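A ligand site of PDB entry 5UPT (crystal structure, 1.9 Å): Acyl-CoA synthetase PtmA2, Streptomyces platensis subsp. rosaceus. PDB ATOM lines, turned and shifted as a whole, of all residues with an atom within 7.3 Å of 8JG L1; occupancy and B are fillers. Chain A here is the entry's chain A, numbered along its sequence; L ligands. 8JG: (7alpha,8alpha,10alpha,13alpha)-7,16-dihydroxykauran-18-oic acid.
OH of Tyr 88 lies within hydrogen-bond range of O2 of 8JG L1, at 2.6 Å.
An oxygen (O2) of 8JG L1 lies within salt-bridge range of the guanidinium group (NH2) of Arg 90.
An oxygen (O) of 8JG L1 lies within hydrogen-bond range of the side-chain sulfur (SD) of Met 262 (3.5 Å).
A ring nitrogen (NE2) of His 218 is in hydrogen-bond range of an oxygen (O3) of 8JG L2, at 3.0 Å.
The side-chain hydroxyl (OG) of Ser 498 is in hydrogen-bond range of the side-chain hydroxyl (OG1) of Thr 496.
A ring nitrogen (ND1) of His 218 is in hydrogen-bond range of the backbone NH (N) of Gly 220, 3.1 Å away.
Phe 217 touches 8JG L1 (CE1 to C13, 3.4 Å).
CE1 of His 218 touches C of 8JG L1 (3.9 Å).
Ser 498 touches 8JG L1 (CB to C10, 3.5 Å).
Hydrophobic or aromatic side chains that line 8JG L1: Tyr 88, Phe 217, His 218 and Met 262.
Of the 18 residues printed, 6 come within 4 Å of 8JG L1.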
ATOM      1  N   TYR A  88     -12.758  11.928  -4.545  1.00  0.00           N
ATOM      2  CA  TYR A  88     -11.449  12.479  -4.233  1.00  0.00           C
ATOM      3  C   TYR A  88     -10.858  13.028  -5.497  1.00  0.00           C
ATOM      4  O   TYR A  88     -10.416  12.286  -6.371  1.00  0.00           O
ATOM      5  CB  TYR A  88     -10.602  11.330  -3.643  1.00  0.00           C
ATOM      6  CG  TYR A  88      -9.225  11.673  -3.211  1.00  0.00           C
ATOM      7  CD1 TYR A  88      -8.993  12.777  -2.427  1.00  0.00           C
ATOM      8  CD2 TYR A  88      -8.144  10.832  -3.509  1.00  0.00           C
ATOM      9  CE1 TYR A  88      -7.714  13.091  -1.991  1.00  0.00           C
ATOM     10  CE2 TYR A  88      -6.860  11.116  -3.074  1.00  0.00           C
ATOM     11  CZ  TYR A  88      -6.650  12.258  -2.301  1.00  0.00           C
ATOM     12  OH  TYR A  88      -5.389  12.609  -1.847  1.00  0.00           O
ATOM     13  N   TRP A  89     -10.822  14.346  -5.602  1.00  0.00           N
ATOM     14  CA  TRP A  89     -10.414  14.987  -6.826  1.00  0.00           C
ATOM     15  C   TRP A  89      -8.936  14.778  -7.136  1.00  0.00           C
ATOM     16  O   TRP A  89      -8.506  15.042  -8.240  1.00  0.00           O
ATOM     17  CB  TRP A  89     -10.770  16.473  -6.851  1.00  0.00           C
ATOM     18  CG  TRP A  89     -10.128  17.296  -5.789  1.00  0.00           C
ATOM     19  CD1 TRP A  89     -10.670  17.672  -4.595  1.00  0.00           C
ATOM     20  CD2 TRP A  89      -8.834  17.890  -5.845  1.00  0.00           C
ATOM     21  NE1 TRP A  89      -9.788  18.449  -3.891  1.00  0.00           N
ATOM     22  CE2 TRP A  89      -8.651  18.597  -4.633  1.00  0.00           C
ATOM     23  CE3 TRP A  89      -7.829  17.924  -6.804  1.00  0.00           C
ATOM     24  CZ2 TRP A  89      -7.486  19.300  -4.357  1.00  0.00           C
ATOM     25  CZ3 TRP A  89      -6.672  18.622  -6.526  1.00  0.00           C
ATOM     26  CH2 TRP A  89      -6.507  19.279  -5.307  1.00  0.00           C
ATOM     27  N   ARG A  90      -8.173  14.290  -6.173  1.00  0.00           N
ATOM     28  CA  ARG A  90      -6.753  13.989  -6.429  1.00  0.00           C
ATOM     29  C   ARG A  90      -6.534  12.544  -6.850  1.00  0.00           C
ATOM     30  O   ARG A  90      -5.389  12.140  -6.985  1.00  0.00           O
ATOM     31  CB  ARG A  90      -5.910  14.266  -5.188  1.00  0.00           C
ATOM     32  CG  ARG A  90      -5.846  15.734  -4.771  1.00  0.00           C
ATOM     33  CD  ARG A  90      -5.337  15.886  -3.331  1.00  0.00           C
ATOM     34  NE  ARG A  90      -4.482  17.053  -3.167  1.00  0.00           N
ATOM     35  CZ  ARG A  90      -3.627  17.246  -2.158  1.00  0.00           C
ATOM     36  NH1 ARG A  90      -2.903  18.355  -2.122  1.00  0.00           N
ATOM     37  NH2 ARG A  90      -3.498  16.352  -1.175  1.00  0.00           N
ATOM     38  N   GLY A 214     -12.325  22.966   4.219  1.00  0.00           N
ATOM     39  CA  GLY A 214     -11.919  21.542   4.289  1.00  0.00           C
ATOM     40  C   GLY A 214     -12.413  20.792   3.049  1.00  0.00           C
ATOM     41  O   GLY A 214     -13.358  21.250   2.392  1.00  0.00           O
ATOM     42  N   PRO A 215     -11.824  19.651   2.708  1.00  0.00           N
ATOM     43  CA  PRO A 215     -12.313  18.981   1.497  1.00  0.00           C
ATOM     44  C   PRO A 215     -13.644  18.290   1.683  1.00  0.00           C
ATOM     45  O   PRO A 215     -13.820  17.509   2.633  1.00  0.00           O
ATOM     46  CB  PRO A 215     -11.234  17.918   1.229  1.00  0.00           C
ATOM     47  CG  PRO A 215     -10.665  17.628   2.577  1.00  0.00           C
ATOM     48  CD  PRO A 215     -10.673  18.930   3.311  1.00  0.00           C
ATOM     49  N   PHE A 217     -14.775  15.908   0.045  1.00  0.00           N
ATOM     50  CA  PHE A 217     -14.617  14.455  -0.127  1.00  0.00           C
ATOM     51  C   PHE A 217     -14.350  13.725   1.179  1.00  0.00           C
ATOM     52  O   PHE A 217     -14.277  12.488   1.217  1.00  0.00           O
ATOM     53  CB  PHE A 217     -13.552  14.094  -1.162  1.00  0.00           C
ATOM     54  CG  PHE A 217     -12.167  14.571  -0.833  1.00  0.00           C
ATOM     55  CD1 PHE A 217     -11.439  14.017   0.210  1.00  0.00           C
ATOM     56  CD2 PHE A 217     -11.561  15.512  -1.637  1.00  0.00           C
ATOM     57  CE1 PHE A 217     -10.158  14.421   0.470  1.00  0.00           C
ATOM     58  CE2 PHE A 217     -10.249  15.942  -1.387  1.00  0.00           C
ATOM     59  CZ  PHE A 217      -9.555  15.391  -0.318  1.00  0.00           C
ATOM     60  N   HIS A 218     -14.210  14.504   2.242  1.00  0.00           N
ATOM     61  CA  HIS A 218     -13.884  13.964   3.575  1.00  0.00           C
ATOM     62  C   HIS A 218     -14.890  14.469   4.608  1.00  0.00           C
ATOM     63  O   HIS A 218     -15.411  15.570   4.491  1.00  0.00           O
ATOM     64  CB  HIS A 218     -12.436  14.382   3.866  1.00  0.00           C
ATOM     65  CG  HIS A 218     -11.928  14.018   5.226  1.00  0.00           C
ATOM     66  ND1 HIS A 218     -12.044  14.850   6.307  1.00  0.00           N
ATOM     67  CD2 HIS A 218     -11.207  12.945   5.662  1.00  0.00           C
ATOM     68  CE1 HIS A 218     -11.509  14.278   7.379  1.00  0.00           C
ATOM     69  NE2 HIS A 218     -10.968  13.131   7.001  1.00  0.00           N
ATOM     70  N   ILE A 219     -15.151  13.651   5.639  1.00  0.00           N
ATOM     71  CA  ILE A 219     -16.251  13.867   6.566  1.00  0.00           C
ATOM     72  C   ILE A 219     -16.010  15.120   7.447  1.00  0.00           C
ATOM     73  O   ILE A 219     -16.972  15.711   7.915  1.00  0.00           O
ATOM     74  CB  ILE A 219     -16.475  12.612   7.415  1.00  0.00           C
ATOM     75  CG1 ILE A 219     -17.752  12.671   8.223  1.00  0.00           C
ATOM     76  CG2 ILE A 219     -15.297  12.365   8.351  1.00  0.00           C
ATOM     77  CD1 ILE A 219     -19.019  12.798   7.458  1.00  0.00           C
ATOM     78  N   GLY A 220     -14.747  15.486   7.665  1.00  0.00           N
ATOM     79  CA  GLY A 220     -14.362  16.599   8.546  1.00  0.00           C
ATOM     80  C   GLY A 220     -15.127  17.907   8.265  1.00  0.00           C
ATOM     81  O   GLY A 220     -15.713  18.497   9.158  1.00  0.00           O
ATOM     82  N   ASN A 221     -15.089  18.343   7.028  1.00  0.00           N
ATOM     83  CA  ASN A 221     -15.707  19.611   6.628  1.00  0.00           C
ATOM     84  C   ASN A 221     -17.236  19.585   6.751  1.00  0.00           C
ATOM     85  O   ASN A 221     -17.856  20.615   7.078  1.00  0.00           O
ATOM     86  CB  ASN A 221     -15.323  19.939   5.183  1.00  0.00           C
ATOM     87  CG  ASN A 221     -15.824  21.299   4.737  1.00  0.00           C
ATOM     88  OD1 ASN A 221     -15.140  22.283   4.936  1.00  0.00           O
ATOM     89  ND2 ASN A 221     -16.998  21.354   4.058  1.00  0.00           N
ATOM     90  N   PHE A 260     -12.650  25.519   8.464  1.00  0.00           N
ATOM     91  CA  PHE A 260     -11.895  24.255   8.655  1.00  0.00           C
ATOM     92  C   PHE A 260     -10.477  24.504   8.188  1.00  0.00           C
ATOM     93  O   PHE A 260     -10.239  24.596   6.959  1.00  0.00           O
ATOM     94  CB  PHE A 260     -12.554  23.133   7.849  1.00  0.00           C
ATOM     95  CG  PHE A 260     -12.043  21.775   8.166  1.00  0.00           C
ATOM     96  CD1 PHE A 260     -12.751  20.939   8.985  1.00  0.00           C
ATOM     97  CD2 PHE A 260     -10.842  21.341   7.639  1.00  0.00           C
ATOM     98  CE1 PHE A 260     -12.304  19.669   9.276  1.00  0.00           C
ATOM     99  CE2 PHE A 260     -10.362  20.051   7.919  1.00  0.00           C
ATOM    100  CZ  PHE A 260     -11.119  19.221   8.730  1.00  0.00           C
ATOM    101  N   MET A 262      -6.176  23.855   9.112  1.00  0.00           N
ATOM    102  CA  MET A 262      -5.128  23.093   9.819  1.00  0.00           C
ATOM    103  C   MET A 262      -4.055  24.096  10.236  1.00  0.00           C
ATOM    104  O   MET A 262      -3.970  25.172   9.641  1.00  0.00           O
ATOM    105  CB  MET A 262      -4.654  21.970   8.900  1.00  0.00           C
ATOM    106  CG  MET A 262      -5.711  20.864   8.648  1.00  0.00           C
ATOM    107  SD  MET A 262      -6.421  20.088  10.339  1.00  0.00           S
ATOM    108  CE  MET A 262      -8.114  21.061  10.385  1.00  0.00           C
ATOM    109  N   PRO A 263      -3.222  23.785  11.254  1.00  0.00           N
ATOM    110  CA  PRO A 263      -2.239  24.751  11.709  1.00  0.00           C
ATOM    111  C   PRO A 263      -1.286  25.364  10.647  1.00  0.00           C
ATOM    112  O   PRO A 263      -0.986  26.535  10.770  1.00  0.00           O
ATOM    113  CB  PRO A 263      -1.433  23.977  12.793  1.00  0.00           C
ATOM    114  CG  PRO A 263      -2.489  23.037  13.344  1.00  0.00           C
ATOM    115  CD  PRO A 263      -3.284  22.614  12.128  1.00  0.00           C
ATOM    116  N   THR A 496       4.669   8.098   4.648  1.00  0.00           N
ATOM    117  CA  THR A 496       4.318   8.061   3.235  1.00  0.00           C
ATOM    118  C   THR A 496       4.237   9.499   2.720  1.00  0.00           C
ATOM    119  O   THR A 496       4.275  10.475   3.502  1.00  0.00           O
ATOM    120  CB  THR A 496       2.971   7.390   3.031  1.00  0.00           C
ATOM    121  OG1 THR A 496       1.974   8.168   3.708  1.00  0.00           O
ATOM    122  CG2 THR A 496       2.992   5.970   3.603  1.00  0.00           C
ATOM    123  N   VAL A 497       4.073   9.641   1.412  1.00  0.00           N
ATOM    124  CA  VAL A 497       3.842  10.987   0.855  1.00  0.00           C
ATOM    125  C   VAL A 497       2.636  11.663   1.504  1.00  0.00           C
ATOM    126  O   VAL A 497       2.607  12.874   1.646  1.00  0.00           O
ATOM    127  CB  VAL A 497       3.699  10.985  -0.688  1.00  0.00           C
ATOM    128  CG1 VAL A 497       5.027  10.591  -1.335  1.00  0.00           C
ATOM    129  CG2 VAL A 497       2.542  10.086  -1.150  1.00  0.00           C
ATOM    130  N   SER A 498       1.649  10.868   1.937  1.00  0.00           N
ATOM    131  CA  SER A 498       0.469  11.413   2.593  1.00  0.00           C
ATOM    132  C   SER A 498       0.659  11.759   4.078  1.00  0.00           C
ATOM    133  O   SER A 498      -0.284  12.258   4.690  1.00  0.00           O
ATOM    134  CB  SER A 498      -0.672  10.419   2.461  1.00  0.00           C
ATOM    135  OG  SER A 498      -0.535   9.403   3.424  1.00  0.00           O
ATOM    136  N   GLY A 499       1.827  11.485   4.650  1.00  0.00           N
ATOM    137  CA  GLY A 499       2.100  11.770   6.066  1.00  0.00           C
ATOM    138  C   GLY A 499       1.802  10.632   7.048  1.00  0.00           C
ATOM    139  O   GLY A 499       2.043  10.768   8.242  1.00  0.00           O
ATOM    140  N   ALA A 500       1.281   9.506   6.554  1.00  0.00           N
ATOM    141  CA  ALA A 500       1.006   8.354   7.462  1.00  0.00           C
ATOM    142  C   ALA A 500       2.233   7.491   7.702  1.00  0.00           C
ATOM    143  O   ALA A 500       3.171   7.485   6.886  1.00  0.00           O
ATOM    144  CB  ALA A 500      -0.113   7.488   6.883  1.00  0.00           C
HETATM  145  C8  8JG L   1      -5.236  13.746   3.549  1.00  0.00           C
HETATM  146  C7  8JG L   1      -4.134  14.501   4.276  1.00  0.00           C
HETATM  147  C6  8JG L   1      -4.491  14.571   5.760  1.00  0.00           C
HETATM  148  C9  8JG L   1      -4.800  13.194   2.169  1.00  0.00           C
HETATM  149  C10 8JG L   1      -3.549  12.320   2.243  1.00  0.00           C
HETATM  150  C5  8JG L   1      -6.239  15.045   7.428  1.00  0.00           C
HETATM  151  C4  8JG L   1      -5.828  15.282   5.984  1.00  0.00           C
HETATM  152  O   8JG L   1      -6.020  16.983   8.853  1.00  0.00           O
HETATM  153  C1  8JG L   1      -6.877  16.342   7.894  1.00  0.00           C
HETATM  154  C2  8JG L   1      -6.901  17.250   6.672  1.00  0.00           C
HETATM  155  C3  8JG L   1      -5.692  16.792   5.866  1.00  0.00           C
HETATM  156  C12 8JG L   1      -5.906  12.291   1.623  1.00  0.00           C
HETATM  157  C17 8JG L   1      -6.934  14.769   5.065  1.00  0.00           C
HETATM  158  C16 8JG L   1      -6.514  15.835   2.748  1.00  0.00           C
HETATM  159  C18 8JG L   1      -8.238  15.605   5.267  1.00  0.00           C
HETATM  160  O2  8JG L   1      -5.133  14.400   0.060  1.00  0.00           O
HETATM  161  C19 8JG L   1      -8.112  17.040   5.783  1.00  0.00           C
HETATM  162  C15 8JG L   1      -6.547  14.539   3.573  1.00  0.00           C
HETATM  163  C14 8JG L   1      -7.615  13.603   3.000  1.00  0.00           C
HETATM  164  C13 8JG L   1      -7.275  12.963   1.657  1.00  0.00           C
HETATM  165  O3  8JG L   1      -3.599  15.137   1.455  1.00  0.00           O
HETATM  166  C11 8JG L   1      -4.466  14.310   1.204  1.00  0.00           C
HETATM  167  O1  8JG L   1      -3.438  15.281   6.427  1.00  0.00           O
HETATM  168  C   8JG L   1      -8.224  16.086   8.572  1.00  0.00           C
HETATM  169  C8  8JG L   2     -10.521  12.529  12.364  1.00  0.00           C
HETATM  170  C7  8JG L   2      -9.130  13.147  12.269  1.00  0.00           C
HETATM  171  C6  8JG L   2      -8.929  14.180  13.375  1.00  0.00           C
HETATM  172  C9  8JG L   2     -10.678  11.219  11.543  1.00  0.00           C
HETATM  173  C10 8JG L   2      -9.554  10.204  11.869  1.00  0.00           C
HETATM  174  C5  8JG L   2      -9.948  16.078  14.675  1.00  0.00           C
HETATM  175  C4  8JG L   2      -9.988  15.298  13.344  1.00  0.00           C
HETATM  176  O   8JG L   2      -8.779  18.158  14.382  1.00  0.00           O
HETATM  177  C1  8JG L   2     -10.065  17.559  14.273  1.00  0.00           C
HETATM  178  C2  8JG L   2     -10.418  17.576  12.791  1.00  0.00           C
HETATM  179  C3  8JG L   2      -9.633  16.361  12.296  1.00  0.00           C
HETATM  180  C12 8JG L   2     -11.986  10.602  12.020  1.00  0.00           C
HETATM  181  C17 8JG L   2     -11.422  14.766  13.148  1.00  0.00           C
HETATM  182  C16 8JG L   2     -11.686  14.148  10.709  1.00  0.00           C
HETATM  183  C18 8JG L   2     -12.421  15.926  12.918  1.00  0.00           C
HETATM  184  O2  8JG L   2     -11.661  10.901   9.263  1.00  0.00           O
HETATM  185  C19 8JG L   2     -11.882  17.306  12.457  1.00  0.00           C
HETATM  186  C15 8JG L   2     -11.632  13.581  12.144  1.00  0.00           C
HETATM  187  C14 8JG L   2     -12.977  12.901  12.474  1.00  0.00           C
HETATM  188  C13 8JG L   2     -13.185  11.553  11.850  1.00  0.00           C
HETATM  189  O3  8JG L   2      -9.734  11.922   9.395  1.00  0.00           O
HETATM  190  C11 8JG L   2     -10.665  11.372  10.008  1.00  0.00           C
HETATM  191  O1  8JG L   2      -7.616  14.687  13.158  1.00  0.00           O
HETATM  192  C   8JG L   2     -10.992  18.372  15.142  1.00  0.00           C
HETATM  193  C8  8JG L   3      -5.073  19.919   1.704  1.00  0.00           C
HETATM  194  C7  8JG L   3      -3.758  19.860   0.933  1.00  0.00           C
HETATM  195  C6  8JG L   3      -2.740  19.093   1.779  1.00  0.00           C
HETATM  196  C9  8JG L   3      -6.334  20.140   0.827  1.00  0.00           C
HETATM  197  C10 8JG L   3      -6.444  19.032  -0.243  1.00  0.00           C
HETATM  198  C5  8JG L   3      -1.725  18.808   4.057  1.00  0.00           C
HETATM  199  C4  8JG L   3      -2.504  19.750   3.139  1.00  0.00           C
HETATM  200  O   8JG L   3       0.617  19.421   4.291  1.00  0.00           O
HETATM  201  C1  8JG L   3      -0.707  19.660   4.812  1.00  0.00           C
HETATM  202  C2  8JG L   3      -1.115  21.095   4.443  1.00  0.00           C
HETATM  203  C3  8JG L   3      -1.603  20.970   3.015  1.00  0.00           C
HETATM  204  C12 8JG L   3      -7.538  19.979   1.741  1.00  0.00           C
HETATM  205  C17 8JG L   3      -3.836  20.103   3.857  1.00  0.00           C
HETATM  206  C16 8JG L   3      -4.714  22.237   2.718  1.00  0.00           C
HETATM  207  C18 8JG L   3      -3.549  20.830   5.192  1.00  0.00           C
HETATM  208  O2  8JG L   3      -7.406  22.319   0.061  1.00  0.00           O
HETATM  209  C19 8JG L   3      -2.257  21.684   5.273  1.00  0.00           C
HETATM  210  C15 8JG L   3      -4.946  20.742   2.990  1.00  0.00           C
HETATM  211  C14 8JG L   3      -6.247  20.571   3.801  1.00  0.00           C
HETATM  212  C13 8JG L   3      -7.475  20.886   2.966  1.00  0.00           C
HETATM  213  O3  8JG L   3      -5.398  21.767  -0.593  1.00  0.00           O
HETATM  214  C11 8JG L   3      -6.363  21.459   0.082  1.00  0.00           C
HETATM  215  O1  8JG L   3      -1.517  19.022   1.040  1.00  0.00           O
HETATM  216  C   8JG L   3      -0.655  19.360   6.313  1.00  0.00           C
